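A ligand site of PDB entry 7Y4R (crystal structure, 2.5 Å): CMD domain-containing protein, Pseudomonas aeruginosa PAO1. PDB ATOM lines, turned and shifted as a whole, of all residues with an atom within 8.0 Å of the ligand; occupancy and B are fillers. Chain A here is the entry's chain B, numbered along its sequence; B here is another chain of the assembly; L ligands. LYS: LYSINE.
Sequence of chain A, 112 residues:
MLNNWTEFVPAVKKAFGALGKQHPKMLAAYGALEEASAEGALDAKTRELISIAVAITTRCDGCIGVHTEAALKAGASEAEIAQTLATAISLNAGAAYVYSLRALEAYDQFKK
The backbone carbonyl oxygen (O) of Asp 108 lies within hydrogen-bond range of a nitrogen (N) of the ligand (2.9 Å).
N of Phe 110 sits close to N of the ligand (3.4 Å).
A nitrogen (N) of the ligand lies within hydrogen-bond range of the backbone carbonyl oxygen (O) of Tyr 107 (3.1 Å).
O of Ala 76 of chain B sits at hydrogen-bond distance from OH of Tyr 107 (2.5 Å).
The side-chain carboxylate (OE2) of Glu 105 sits at hydrogen-bond distance from the side-chain amide nitrogen (NE2) of Gln 109, 3.2 Å away.
Residues that only touch the ligand: Leu 72 of chain B (3.7 Å) and Gln 109 (3.8 Å).
Five residues have an atom within 4 Å of the ligand: Tyr 107, Asp 108, Gln 109, Phe 110 and Leu 72 of chain B.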
ATOM      1  N   LEU A 104      23.241 -32.482   8.930  1.00  0.00           N
ATOM      2  CA  LEU A 104      23.037 -32.598   7.490  1.00  0.00           C
ATOM      3  C   LEU A 104      21.748 -31.899   7.061  1.00  0.00           C
ATOM      4  O   LEU A 104      21.721 -31.209   6.036  1.00  0.00           O
ATOM      5  CB  LEU A 104      23.007 -34.069   7.081  1.00  0.00           C
ATOM      6  CG  LEU A 104      24.348 -34.811   7.136  1.00  0.00           C
ATOM      7  CD1 LEU A 104      24.158 -36.281   6.816  1.00  0.00           C
ATOM      8  CD2 LEU A 104      25.359 -34.172   6.187  1.00  0.00           C
ATOM      9  N   GLU A 105      20.675 -32.061   7.846  1.00  0.00           N
ATOM     10  CA  GLU A 105      19.442 -31.340   7.552  1.00  0.00           C
ATOM     11  C   GLU A 105      19.641 -29.839   7.697  1.00  0.00           C
ATOM     12  O   GLU A 105      19.075 -29.053   6.917  1.00  0.00           O
ATOM     13  CB  GLU A 105      18.314 -31.829   8.461  1.00  0.00           C
ATOM     14  CG  GLU A 105      16.944 -31.204   8.226  1.00  0.00           C
ATOM     15  CD  GLU A 105      16.563 -31.121   6.749  1.00  0.00           C
ATOM     16  OE1 GLU A 105      16.118 -32.139   6.199  1.00  0.00           O
ATOM     17  OE2 GLU A 105      16.680 -30.025   6.170  1.00  0.00           O
ATOM     18  N   ALA A 106      20.440 -29.411   8.679  1.00  0.00           N
ATOM     19  CA  ALA A 106      20.739 -27.995   8.829  1.00  0.00           C
ATOM     20  C   ALA A 106      21.449 -27.461   7.591  1.00  0.00           C
ATOM     21  O   ALA A 106      21.069 -26.412   7.054  1.00  0.00           O
ATOM     22  CB  ALA A 106      21.577 -27.759  10.082  1.00  0.00           C
ATOM     23  N   TYR A 107      22.466 -28.173   7.113  1.00  0.00           N
ATOM     24  CA  TYR A 107      23.191 -27.727   5.929  1.00  0.00           C
ATOM     25  C   TYR A 107      22.301 -27.730   4.691  1.00  0.00           C
ATOM     26  O   TYR A 107      22.427 -26.852   3.837  1.00  0.00           O
ATOM     27  CB  TYR A 107      24.410 -28.623   5.705  1.00  0.00           C
ATOM     28  CG  TYR A 107      25.266 -28.233   4.518  1.00  0.00           C
ATOM     29  CD1 TYR A 107      26.107 -27.122   4.582  1.00  0.00           C
ATOM     30  CD2 TYR A 107      25.242 -28.974   3.347  1.00  0.00           C
ATOM     31  CE1 TYR A 107      26.890 -26.760   3.507  1.00  0.00           C
ATOM     32  CE2 TYR A 107      26.026 -28.618   2.264  1.00  0.00           C
ATOM     33  CZ  TYR A 107      26.844 -27.508   2.354  1.00  0.00           C
ATOM     34  OH  TYR A 107      27.627 -27.146   1.278  1.00  0.00           O
ATOM     35  N   ASP A 108      21.394 -28.705   4.592  1.00  0.00           N
ATOM     36  CA  ASP A 108      20.493 -28.770   3.449  1.00  0.00           C
ATOM     37  C   ASP A 108      19.493 -27.625   3.419  1.00  0.00           C
ATOM     38  O   ASP A 108      18.998 -27.275   2.352  1.00  0.00           O
ATOM     39  CB  ASP A 108      19.755 -30.112   3.454  1.00  0.00           C
ATOM     40  CG  ASP A 108      18.729 -30.229   2.343  1.00  0.00           C
ATOM     41  OD1 ASP A 108      19.129 -30.380   1.175  1.00  0.00           O
ATOM     42  OD2 ASP A 108      17.520 -30.166   2.642  1.00  0.00           O
ATOM     43  N   GLN A 109      19.197 -27.019   4.569  1.00  0.00           N
ATOM     44  CA  GLN A 109      18.194 -25.966   4.662  1.00  0.00           C
ATOM     45  C   GLN A 109      18.756 -24.569   4.427  1.00  0.00           C
ATOM     46  O   GLN A 109      17.988 -23.655   4.117  1.00  0.00           O
ATOM     47  CB  GLN A 109      17.511 -26.004   6.024  1.00  0.00           C
ATOM     48  CG  GLN A 109      16.228 -26.825   6.056  1.00  0.00           C
ATOM     49  CD  GLN A 109      15.613 -26.886   7.431  1.00  0.00           C
ATOM     50  OE1 GLN A 109      15.855 -26.013   8.278  1.00  0.00           O
ATOM     51  NE2 GLN A 109      14.819 -27.923   7.683  1.00  0.00           N
ATOM     52  N   PHE A 110      20.069 -24.382   4.575  1.00  0.00           N
ATOM     53  CA  PHE A 110      20.656 -23.050   4.482  1.00  0.00           C
ATOM     54  C   PHE A 110      21.007 -22.689   3.038  1.00  0.00           C
ATOM     55  O   PHE A 110      21.860 -21.836   2.796  1.00  0.00           O
ATOM     56  CB  PHE A 110      21.897 -22.954   5.365  1.00  0.00           C
ATOM     57  CG  PHE A 110      21.588 -22.713   6.813  1.00  0.00           C
ATOM     58  CD1 PHE A 110      20.884 -21.590   7.199  1.00  0.00           C
ATOM     59  CD2 PHE A 110      22.003 -23.616   7.775  1.00  0.00           C
ATOM     60  CE1 PHE A 110      20.598 -21.363   8.527  1.00  0.00           C
ATOM     61  CE2 PHE A 110      21.716 -23.397   9.110  1.00  0.00           C
ATOM     62  CZ  PHE A 110      21.014 -22.273   9.483  1.00  0.00           C
ATOM     63  N   THR B   6      16.731 -22.624   9.632  1.00  0.00           N
ATOM     64  CA  THR B   6      16.843 -21.245   9.190  1.00  0.00           C
ATOM     65  C   THR B   6      16.101 -20.280  10.105  1.00  0.00           C
ATOM     66  O   THR B   6      16.362 -19.072  10.047  1.00  0.00           O
ATOM     67  CB  THR B   6      16.307 -21.108   7.756  1.00  0.00           C
ATOM     68  OG1 THR B   6      15.134 -21.911   7.609  1.00  0.00           O
ATOM     69  CG2 THR B   6      17.352 -21.570   6.747  1.00  0.00           C
ATOM     70  N   LEU B  72      28.999 -23.495   5.631  1.00  0.00           N
ATOM     71  CA  LEU B  72      28.556 -23.213   4.266  1.00  0.00           C
ATOM     72  C   LEU B  72      29.062 -21.854   3.816  1.00  0.00           C
ATOM     73  O   LEU B  72      29.558 -21.709   2.689  1.00  0.00           O
ATOM     74  CB  LEU B  72      27.025 -23.271   4.194  1.00  0.00           C
ATOM     75  CG  LEU B  72      26.295 -22.986   2.876  1.00  0.00           C
ATOM     76  CD1 LEU B  72      27.083 -23.444   1.646  1.00  0.00           C
ATOM     77  CD2 LEU B  72      24.913 -23.623   2.893  1.00  0.00           C
ATOM     78  N   LYS B  73      28.959 -20.842   4.689  1.00  0.00           N
ATOM     79  CA  LYS B  73      29.454 -19.517   4.336  1.00  0.00           C
ATOM     80  C   LYS B  73      30.959 -19.533   4.095  1.00  0.00           C
ATOM     81  O   LYS B  73      31.475 -18.688   3.352  1.00  0.00           O
ATOM     82  CB  LYS B  73      29.104 -18.505   5.439  1.00  0.00           C
ATOM     83  CG  LYS B  73      27.625 -18.148   5.539  1.00  0.00           C
ATOM     84  CD  LYS B  73      26.893 -18.380   4.227  1.00  0.00           C
ATOM     85  CE  LYS B  73      25.423 -18.016   4.336  1.00  0.00           C
ATOM     86  NZ  LYS B  73      24.977 -17.159   3.196  1.00  0.00           N
ATOM     87  N   ALA B  76      32.119 -24.832   2.476  1.00  0.00           N
ATOM     88  CA  ALA B  76      32.246 -26.264   2.750  1.00  0.00           C
ATOM     89  C   ALA B  76      31.194 -27.030   1.962  1.00  0.00           C
ATOM     90  O   ALA B  76      29.998 -26.714   2.049  1.00  0.00           O
ATOM     91  CB  ALA B  76      32.111 -26.549   4.243  1.00  0.00           C
ATOM     92  N   SER B  77      31.637 -28.026   1.205  1.00  0.00           N
ATOM     93  CA  SER B  77      30.724 -28.849   0.430  1.00  0.00           C
ATOM     94  C   SER B  77      30.007 -29.846   1.341  1.00  0.00           C
ATOM     95  O   SER B  77      30.288 -29.956   2.534  1.00  0.00           O
ATOM     96  CB  SER B  77      31.468 -29.576  -0.684  1.00  0.00           C
ATOM     97  OG  SER B  77      32.465 -30.445  -0.162  1.00  0.00           O
ATOM     98  N   GLU B  78      29.075 -30.602   0.746  1.00  0.00           N
ATOM     99  CA  GLU B  78      28.282 -31.542   1.530  1.00  0.00           C
ATOM    100  C   GLU B  78      29.118 -32.739   1.952  1.00  0.00           C
ATOM    101  O   GLU B  78      28.935 -33.271   3.056  1.00  0.00           O
ATOM    102  CB  GLU B  78      27.050 -31.976   0.736  1.00  0.00           C
ATOM    103  CG  GLU B  78      25.937 -32.554   1.606  1.00  0.00           C
ATOM    104  CD  GLU B  78      25.986 -34.066   1.673  1.00  0.00           C
ATOM    105  OE1 GLU B  78      26.896 -34.666   1.069  1.00  0.00           O
ATOM    106  OE2 GLU B  78      25.098 -34.660   2.325  1.00  0.00           O
HETATM  107  N   LYS L   1      21.019 -25.320   1.490  1.00  0.00           N
HETATM  108  CA  LYS L   1      21.509 -25.029   0.150  1.00  0.00           C
HETATM  109  C   LYS L   1      22.233 -26.240  -0.425  1.00  0.00           C
HETATM  110  O   LYS L   1      23.171 -26.760   0.183  1.00  0.00           O
HETATM  111  CB  LYS L   1      22.447 -23.815   0.160  1.00  0.00           C
HETATM  112  CG  LYS L   1      21.916 -22.585  -0.569  1.00  0.00           C
HETATM  113  CD  LYS L   1      20.508 -22.799  -1.121  1.00  0.00           C
HETATM  114  CE  LYS L   1      20.313 -22.079  -2.447  1.00  0.00           C
HETATM  115  NZ  LYS L   1      21.446 -21.165  -2.754  1.00  0.00           N
